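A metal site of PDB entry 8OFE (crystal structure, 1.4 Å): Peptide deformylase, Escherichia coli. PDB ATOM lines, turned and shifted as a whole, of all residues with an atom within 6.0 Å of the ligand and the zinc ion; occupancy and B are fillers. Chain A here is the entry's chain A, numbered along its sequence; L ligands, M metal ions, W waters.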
ATOM      1  N   GLU A  44      -9.533 -12.721  -2.873  1.00  0.00           N
ATOM      2  CA  GLU A  44     -10.343 -12.455  -4.064  1.00  0.00           C
ATOM      3  C   GLU A  44      -9.645 -12.862  -5.349  1.00  0.00           C
ATOM      4  O   GLU A  44     -10.173 -12.588  -6.448  1.00  0.00           O
ATOM      5  CB  GLU A  44     -10.733 -10.979  -4.110  1.00  0.00           C
ATOM      6  CG  GLU A  44     -11.511 -10.536  -2.850  1.00  0.00           C
ATOM      7  CD  GLU A  44     -12.892  -9.975  -3.186  1.00  0.00           C
ATOM      8  OE1 GLU A  44     -13.048  -9.357  -4.263  1.00  0.00           O
ATOM      9  OE2 GLU A  44     -13.819 -10.190  -2.381  1.00  0.00           O
ATOM     10  N   GLU A  45      -8.479 -13.490  -5.234  1.00  0.00           N
ATOM     11  CA  GLU A  45      -7.699 -13.969  -6.371  1.00  0.00           C
ATOM     12  C   GLU A  45      -7.217 -12.823  -7.260  1.00  0.00           C
ATOM     13  O   GLU A  45      -7.129 -12.984  -8.485  1.00  0.00           O
ATOM     14  CB  GLU A  45      -8.443 -15.057  -7.171  1.00  0.00           C
ATOM     15  CG  GLU A  45      -8.643 -16.310  -6.328  1.00  0.00           C
ATOM     16  CD  GLU A  45      -9.502 -17.345  -6.945  1.00  0.00           C
ATOM     17  OE1 GLU A  45      -9.808 -17.266  -8.146  1.00  0.00           O
ATOM     18  OE2 GLU A  45      -9.865 -18.256  -6.197  1.00  0.00           O
ATOM     19  N   GLY A  46      -6.931 -11.680  -6.671  1.00  0.00           N
ATOM     20  CA  GLY A  46      -6.436 -10.556  -7.427  1.00  0.00           C
ATOM     21  C   GLY A  46      -4.931 -10.513  -7.478  1.00  0.00           C
ATOM     22  O   GLY A  46      -4.247 -11.114  -6.650  1.00  0.00           O
ATOM     23  N   ILE A  47      -4.394  -9.717  -8.404  1.00  0.00           N
ATOM     24  CA  ILE A  47      -2.964  -9.432  -8.486  1.00  0.00           C
ATOM     25  C   ILE A  47      -2.651  -8.010  -8.064  1.00  0.00           C
ATOM     26  O   ILE A  47      -1.486  -7.635  -7.995  1.00  0.00           O
ATOM     27  CB  ILE A  47      -2.368  -9.747  -9.869  1.00  0.00           C
ATOM     28  CG1 ILE A  47      -3.041  -8.876 -10.931  1.00  0.00           C
ATOM     29  CG2 ILE A  47      -2.525 -11.210 -10.200  1.00  0.00           C
ATOM     30  CD1 ILE A  47      -2.369  -9.020 -12.287  1.00  0.00           C
ATOM     31  N   GLY A  48      -3.675  -7.204  -7.781  1.00  0.00           N
ATOM     32  CA  GLY A  48      -3.436  -5.886  -7.221  1.00  0.00           C
ATOM     33  C   GLY A  48      -4.675  -5.464  -6.499  1.00  0.00           C
ATOM     34  O   GLY A  48      -5.746  -6.016  -6.721  1.00  0.00           O
ATOM     35  N   LEU A  49      -4.533  -4.440  -5.663  1.00  0.00           N
ATOM     36  CA  LEU A  49      -5.659  -3.867  -4.944  1.00  0.00           C
ATOM     37  C   LEU A  49      -5.249  -2.470  -4.510  1.00  0.00           C
ATOM     38  O   LEU A  49      -4.150  -2.268  -4.004  1.00  0.00           O
ATOM     39  CB  LEU A  49      -6.000  -4.694  -3.686  1.00  0.00           C
ATOM     40  CG  LEU A  49      -7.292  -4.367  -2.979  1.00  0.00           C
ATOM     41  CD1 LEU A  49      -8.481  -4.727  -3.806  1.00  0.00           C
ATOM     42  CD2 LEU A  49      -7.404  -5.035  -1.599  1.00  0.00           C
ATOM     43  N   ALA A  50      -6.163  -1.512  -4.699  1.00  0.00           N
ATOM     44  CA  ALA A  50      -5.946  -0.137  -4.291  1.00  0.00           C
ATOM     45  C   ALA A  50      -6.812   0.178  -3.083  1.00  0.00           C
ATOM     46  O   ALA A  50      -7.929  -0.340  -2.951  1.00  0.00           O
ATOM     47  CB  ALA A  50      -6.288   0.803  -5.471  1.00  0.00           C
ATOM     48  N   GLN A  53     -10.510   0.860  -3.285  1.00  0.00           N
ATOM     49  CA  GLN A  53     -11.454  -0.243  -3.527  1.00  0.00           C
ATOM     50  C   GLN A  53     -12.011  -0.829  -2.233  1.00  0.00           C
ATOM     51  O   GLN A  53     -12.991  -1.595  -2.283  1.00  0.00           O
ATOM     52  CB  GLN A  53     -10.815  -1.370  -4.320  1.00  0.00           C
ATOM     53  CG  GLN A  53     -10.391  -0.969  -5.758  1.00  0.00           C
ATOM     54  CD  GLN A  53      -9.709  -2.137  -6.441  1.00  0.00           C
ATOM     55  OE1 GLN A  53      -8.516  -2.318  -6.304  1.00  0.00           O
ATOM     56  NE2 GLN A  53     -10.492  -2.937  -7.155  1.00  0.00           N
ATOM     57  N   ILE A  89      -3.895  -5.337 -22.676  1.00  0.00           N
ATOM     58  CA  ILE A  89      -4.428  -6.683 -22.485  1.00  0.00           C
ATOM     59  C   ILE A  89      -5.872  -6.574 -22.035  1.00  0.00           C
ATOM     60  O   ILE A  89      -6.349  -5.498 -21.673  1.00  0.00           O
ATOM     61  CB  ILE A  89      -3.604  -7.481 -21.459  1.00  0.00           C
ATOM     62  CG1 ILE A  89      -3.719  -6.877 -20.035  1.00  0.00           C
ATOM     63  CG2 ILE A  89      -2.165  -7.606 -21.960  1.00  0.00           C
ATOM     64  CD1 ILE A  89      -2.966  -7.712 -18.944  1.00  0.00           C
ATOM     65  N   GLU A  90      -6.539  -7.715 -22.021  1.00  0.00           N
ATOM     66  CA  GLU A  90      -7.878  -7.811 -21.462  1.00  0.00           C
ATOM     67  C   GLU A  90      -7.804  -7.702 -19.960  1.00  0.00           C
ATOM     68  O   GLU A  90      -7.362  -8.633 -19.285  1.00  0.00           O
ATOM     69  CB  GLU A  90      -8.505  -9.158 -21.839  1.00  0.00           C
ATOM     70  CG  GLU A  90      -8.768  -9.262 -23.271  1.00  0.00           C
ATOM     71  CD  GLU A  90     -10.066  -8.659 -23.690  1.00  0.00           C
ATOM     72  OE1 GLU A  90     -10.866  -8.257 -22.820  1.00  0.00           O
ATOM     73  OE2 GLU A  90     -10.300  -8.625 -24.905  1.00  0.00           O
ATOM     74  N   GLU A  91      -8.192  -6.562 -19.404  1.00  0.00           N
ATOM     75  CA  GLU A  91      -8.120  -6.335 -17.961  1.00  0.00           C
ATOM     76  C   GLU A  91      -9.445  -6.663 -17.322  1.00  0.00           C
ATOM     77  O   GLU A  91     -10.485  -6.442 -17.905  1.00  0.00           O
ATOM     78  CB  GLU A  91      -7.796  -4.872 -17.663  1.00  0.00           C
ATOM     79  CG  GLU A  91      -6.456  -4.435 -18.130  1.00  0.00           C
ATOM     80  CD  GLU A  91      -6.090  -3.013 -17.723  1.00  0.00           C
ATOM     81  OE1 GLU A  91      -6.605  -2.471 -16.687  1.00  0.00           O
ATOM     82  OE2 GLU A  91      -5.220  -2.441 -18.398  1.00  0.00           O
ATOM     83  N   GLY A  92      -9.388  -7.218 -16.109  1.00  0.00           N
ATOM     84  CA  GLY A  92     -10.516  -7.291 -15.211  1.00  0.00           C
ATOM     85  C   GLY A  92     -10.259  -6.456 -13.968  1.00  0.00           C
ATOM     86  O   GLY A  92      -9.180  -5.880 -13.805  1.00  0.00           O
ATOM     87  N   CYS A  93     -11.291  -6.328 -13.121  1.00  0.00           N
ATOM     88  CA  CYS A  93     -11.224  -5.475 -11.942  1.00  0.00           C
ATOM     89  C   CYS A  93     -12.127  -6.091 -10.880  1.00  0.00           C
ATOM     90  O   CYS A  93     -13.272  -6.432 -11.172  1.00  0.00           O
ATOM     91  CB  CYS A  93     -11.657  -4.023 -12.245  1.00  0.00           C
ATOM     92  SG  CYS A  93     -11.525  -2.900 -10.846  1.00  0.00           S
ATOM     93  N   LEU A  94     -11.611  -6.185  -9.639  1.00  0.00           N
ATOM     94  CA  LEU A  94     -12.430  -6.738  -8.550  1.00  0.00           C
ATOM     95  C   LEU A  94     -13.649  -5.873  -8.263  1.00  0.00           C
ATOM     96  O   LEU A  94     -14.606  -6.359  -7.633  1.00  0.00           O
ATOM     97  CB  LEU A  94     -11.608  -6.872  -7.274  1.00  0.00           C
ATOM     98  CG  LEU A  94     -10.529  -7.968  -7.286  1.00  0.00           C
ATOM     99  CD1 LEU A  94      -9.633  -7.920  -6.036  1.00  0.00           C
ATOM    100  CD2 LEU A  94     -11.190  -9.355  -7.438  1.00  0.00           C
ATOM    101  N   SER A  95     -13.584  -4.592  -8.653  1.00  0.00           N
ATOM    102  CA  SER A  95     -14.721  -3.685  -8.466  1.00  0.00           C
ATOM    103  C   SER A  95     -15.718  -3.730  -9.617  1.00  0.00           C
ATOM    104  O   SER A  95     -16.766  -3.068  -9.527  1.00  0.00           O
ATOM    105  CB  SER A  95     -14.239  -2.245  -8.241  1.00  0.00           C
ATOM    106  OG  SER A  95     -13.415  -2.172  -7.086  1.00  0.00           O
ATOM    107  N   GLN A  99     -16.328  -8.755 -15.707  1.00  0.00           N
ATOM    108  CA  GLN A  99     -16.196  -8.018 -16.964  1.00  0.00           C
ATOM    109  C   GLN A  99     -14.723  -7.832 -17.310  1.00  0.00           C
ATOM    110  O   GLN A  99     -13.874  -7.658 -16.434  1.00  0.00           O
ATOM    111  CB  GLN A  99     -16.893  -6.674 -16.834  1.00  0.00           C
ATOM    112  CG  GLN A  99     -18.289  -6.732 -16.210  1.00  0.00           C
ATOM    113  CD  GLN A  99     -19.195  -7.770 -16.852  1.00  0.00           C
ATOM    114  OE1 GLN A  99     -19.396  -7.775 -18.067  1.00  0.00           O
ATOM    115  NE2 GLN A  99     -19.731  -8.691 -16.011  1.00  0.00           N
ATOM    116  N   LEU A 128       3.066  -7.034 -17.918  1.00  0.00           N
ATOM    117  CA  LEU A 128       1.952  -7.184 -16.988  1.00  0.00           C
ATOM    118  C   LEU A 128       2.113  -6.289 -15.764  1.00  0.00           C
ATOM    119  O   LEU A 128       1.144  -5.651 -15.314  1.00  0.00           O
ATOM    120  CB  LEU A 128       1.832  -8.658 -16.580  1.00  0.00           C
ATOM    121  CG  LEU A 128       0.718  -8.894 -15.535  1.00  0.00           C
ATOM    122  CD1 LEU A 128      -0.714  -8.551 -16.036  1.00  0.00           C
ATOM    123  CD2 LEU A 128       0.826 -10.362 -15.055  1.00  0.00           C
ATOM    124  N   ILE A 131       1.258  -2.718 -16.510  1.00  0.00           N
ATOM    125  CA  ILE A 131      -0.179  -2.591 -16.698  1.00  0.00           C
ATOM    126  C   ILE A 131      -0.884  -2.550 -15.347  1.00  0.00           C
ATOM    127  O   ILE A 131      -1.741  -1.686 -15.077  1.00  0.00           O
ATOM    128  CB  ILE A 131      -0.678  -3.748 -17.597  1.00  0.00           C
ATOM    129  CG1 ILE A 131      -0.170  -3.530 -19.054  1.00  0.00           C
ATOM    130  CG2 ILE A 131      -2.177  -3.865 -17.572  1.00  0.00           C
ATOM    131  CD1 ILE A 131      -0.323  -4.734 -19.932  1.00  0.00           C
ATOM    132  N   CYS A 132      -0.529  -3.487 -14.457  1.00  0.00           N
ATOM    133  CA  CYS A 132      -1.160  -3.522 -13.159  1.00  0.00           C
ATOM    134  C   CYS A 132      -0.888  -2.251 -12.355  1.00  0.00           C
ATOM    135  O   CYS A 132      -1.808  -1.707 -11.712  1.00  0.00           O
ATOM    136  CB  CYS A 132      -0.643  -4.780 -12.437  1.00  0.00           C
ATOM    137  SG  CYS A 132      -1.298  -4.977 -10.780  1.00  0.00           S
ATOM    138  N   HIS A 135      -3.219   0.415 -13.691  1.00  0.00           N
ATOM    139  CA  HIS A 135      -4.575   0.135 -13.261  1.00  0.00           C
ATOM    140  C   HIS A 135      -4.793   0.539 -11.796  1.00  0.00           C
ATOM    141  O   HIS A 135      -5.787   1.182 -11.443  1.00  0.00           O
ATOM    142  CB  HIS A 135      -4.824  -1.348 -13.510  1.00  0.00           C
ATOM    143  CG  HIS A 135      -6.172  -1.866 -13.102  1.00  0.00           C
ATOM    144  ND1 HIS A 135      -7.062  -2.401 -14.003  1.00  0.00           N
ATOM    145  CD2 HIS A 135      -6.751  -1.984 -11.884  1.00  0.00           C
ATOM    146  CE1 HIS A 135      -8.142  -2.793 -13.353  1.00  0.00           C
ATOM    147  NE2 HIS A 135      -7.968  -2.566 -12.072  1.00  0.00           N
ATOM    148  N   GLU A 136      -3.853   0.197 -10.911  1.00  0.00           N
ATOM    149  CA  GLU A 136      -4.032   0.515  -9.509  1.00  0.00           C
ATOM    150  C   GLU A 136      -3.871   2.010  -9.243  1.00  0.00           C
ATOM    151  O   GLU A 136      -4.607   2.558  -8.420  1.00  0.00           O
ATOM    152  CB  GLU A 136      -3.027  -0.249  -8.635  1.00  0.00           C
ATOM    153  CG  GLU A 136      -3.081  -1.767  -8.842  1.00  0.00           C
ATOM    154  CD  GLU A 136      -4.457  -2.361  -8.695  1.00  0.00           C
ATOM    155  OE1 GLU A 136      -5.341  -1.756  -8.051  1.00  0.00           O
ATOM    156  OE2 GLU A 136      -4.658  -3.449  -9.287  1.00  0.00           O
ATOM    157  N   HIS A 139      -7.009   3.736  -9.847  1.00  0.00           N
ATOM    158  CA  HIS A 139      -8.001   3.651  -8.778  1.00  0.00           C
ATOM    159  C   HIS A 139      -7.823   4.754  -7.752  1.00  0.00           C
ATOM    160  O   HIS A 139      -8.805   5.265  -7.195  1.00  0.00           O
ATOM    161  CB  HIS A 139      -7.877   2.327  -8.016  1.00  0.00           C
ATOM    162  CG  HIS A 139      -8.632   1.195  -8.628  1.00  0.00           C
ATOM    163  ND1 HIS A 139      -9.992   1.238  -8.881  1.00  0.00           N
ATOM    164  CD2 HIS A 139      -8.210  -0.034  -9.043  1.00  0.00           C
ATOM    165  CE1 HIS A 139     -10.373   0.083  -9.393  1.00  0.00           C
ATOM    166  NE2 HIS A 139      -9.320  -0.689  -9.518  1.00  0.00           N
ATOM    167  N   LEU A 144     -11.471   4.060 -13.388  1.00  0.00           N
ATOM    168  CA  LEU A 144     -11.732   2.643 -13.617  1.00  0.00           C
ATOM    169  C   LEU A 144     -11.390   2.297 -15.052  1.00  0.00           C
ATOM    170  O   LEU A 144     -11.475   3.146 -15.942  1.00  0.00           O
ATOM    171  CB  LEU A 144     -13.203   2.308 -13.368  1.00  0.00           C
ATOM    172  CG  LEU A 144     -13.616   2.655 -11.941  1.00  0.00           C
ATOM    173  CD1 LEU A 144     -15.139   2.527 -11.797  1.00  0.00           C
ATOM    174  CD2 LEU A 144     -12.890   1.752 -10.949  1.00  0.00           C
ATOM    175  N   PHE A 145     -11.079   1.033 -15.324  1.00  0.00           N
ATOM    176  CA  PHE A 145     -10.643   0.702 -16.678  1.00  0.00           C
ATOM    177  C   PHE A 145     -11.757   0.958 -17.681  1.00  0.00           C
ATOM    178  O   PHE A 145     -11.488   1.249 -18.855  1.00  0.00           O
ATOM    179  CB  PHE A 145     -10.098  -0.738 -16.800  1.00  0.00           C
ATOM    180  CG  PHE A 145     -11.147  -1.832 -16.868  1.00  0.00           C
ATOM    181  CD1 PHE A 145     -11.808  -2.111 -18.052  1.00  0.00           C
ATOM    182  CD2 PHE A 145     -11.473  -2.577 -15.755  1.00  0.00           C
ATOM    183  CE1 PHE A 145     -12.751  -3.110 -18.120  1.00  0.00           C
ATOM    184  CE2 PHE A 145     -12.388  -3.586 -15.818  1.00  0.00           C
ATOM    185  CZ  PHE A 145     -13.027  -3.860 -16.992  1.00  0.00           C
HETATM  186  C1  LIG L   1      -4.495  -6.686 -15.327  1.00  0.00           C
HETATM  187  C2  LIG L   1      -4.492  -5.321 -14.668  1.00  0.00           C
HETATM  188  C3  LIG L   1      -7.296  -6.650 -10.709  1.00  0.00           C
HETATM  189  C4  LIG L   1      -5.967  -5.992 -11.088  1.00  0.00           C
HETATM  190  C5  LIG L   1      -5.609  -6.199 -12.548  1.00  0.00           C
HETATM  191  C6  LIG L   1      -4.476  -5.361 -13.144  1.00  0.00           C
HETATM  192  C7  LIG L   1      -7.707 -10.268 -13.734  1.00  0.00           C
HETATM  193  C8  LIG L   1      -7.979 -10.077 -12.243  1.00  0.00           C
HETATM  194  C9  LIG L   1      -7.348  -4.076  -8.772  1.00  0.00           C
HETATM  195  C10 LIG L   1      -9.384 -10.710 -10.274  1.00  0.00           C
HETATM  196  C11 LIG L   1      -9.314 -10.708 -11.796  1.00  0.00           C
HETATM  197  C12 LIG L   1     -10.515 -10.005 -12.388  1.00  0.00           C
HETATM  198  C13 LIG L   1      -7.698  -6.432  -9.259  1.00  0.00           C
HETATM  199  C14 LIG L   1      -7.226  -8.155 -10.943  1.00  0.00           C
HETATM  200  N1  LIG L   1      -8.102  -5.038  -9.161  1.00  0.00           N
HETATM  201  N2  LIG L   1      -7.927  -8.647 -11.956  1.00  0.00           N
HETATM  202  N3  LIG L   1      -7.360 -11.516 -14.125  1.00  0.00           N
HETATM  203  O1  LIG L   1      -9.355  -4.620  -9.613  1.00  0.00           O
HETATM  204  O2  LIG L   1      -7.671  -2.944  -8.955  1.00  0.00           O
HETATM  205  O3  LIG L   1      -6.555  -8.853 -10.207  1.00  0.00           O
HETATM  206  O4  LIG L   1      -7.794  -9.343 -14.529  1.00  0.00           O
HETATM  207 ZN    ZN M   1      -9.254  -2.687 -10.380  1.00  0.00          ZN
HETATM  208  O   HOH W   1      -6.421 -13.505 -12.760  1.00  0.00           O
HETATM  209  O   HOH W   2      -8.194 -14.413 -14.588  1.00  0.00           O
HETATM  210  O   HOH W   3      -8.191 -13.958 -10.638  1.00  0.00           O
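An oxygen (O3) of the ligand lies within hydrogen-bond range of the backbone NH (N) of Ile 47, 2.9 Å away.
The backbone NH of Leu 94 sits close to an oxygen (O1) of the ligand (2.7 Å).
O2 of the ligand sits close to OE1 of Gln 53, at 2.9 Å.
The backbone NH (N) of Gly 92 lies within hydrogen-bond range of an oxygen (O4) of the ligand, at 3.1 Å.
The side-chain sulfur (SG) of Cys 93 sits close to the backbone NH (N) of Ser 95, 3.5 Å away.
The side-chain amide oxygen (OE1) of Gln 53 is in hydrogen-bond range of the backbone NH (N) of Ala 50 (3.0 Å).
A ring nitrogen (ND1) of His 135 lies within hydrogen-bond range of the side-chain carboxylate (OE1) of Glu 91 (2.7 Å).
NE2 of Gln 53 is in hydrogen-bond range of OG of Ser 95 (3.0 Å).
The backbone NH of Ala 50 lies within hydrogen-bond range of the side-chain carboxylate of Glu 136 (3.5 Å).
A ring nitrogen (NE2) of His 139 lies close to the side-chain amide nitrogen of Gln 53, 3.5 Å away.
O2 of the ligand sits close to OE1 of Glu 136, 2.8 Å away.
Glu 45 touches the ligand.
Gly 46 touches the ligand (CA to O3, 3.3 Å).
Gly 48 touches the ligand.
CG2 of Ile 131 touches C2 of the ligand, at 3.99 Å.
Cys 132 touches the ligand (CA to C6, 3.8 Å).
Hydrophobic or aromatic side chains that line the ligand: Ile 47, Leu 94, Ile 131, His 135 and His 139.
Within 4 Å of the ligand: Glu 45, Gly 46, Ile 47, Gly 48, Gln 53, Gly 92, Cys 93, Leu 94, Ile 131, Cys 132, His 135, Glu 136 and His 139.
The nearest printed residue that does not touch the ligand is Ile 89 (4.1 Å).
Gln 53 touches the zinc ion.
The zinc ion is bound by O1 of the ligand (2.1 Å), NE2 of His 135 (2.1 Å), O2 of the ligand (2.1 Å), NE2 of His 139 (2.2 Å) and SG of Cys 93 (2.3 Å).
The zinc ion has five donor atoms within binding distance.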
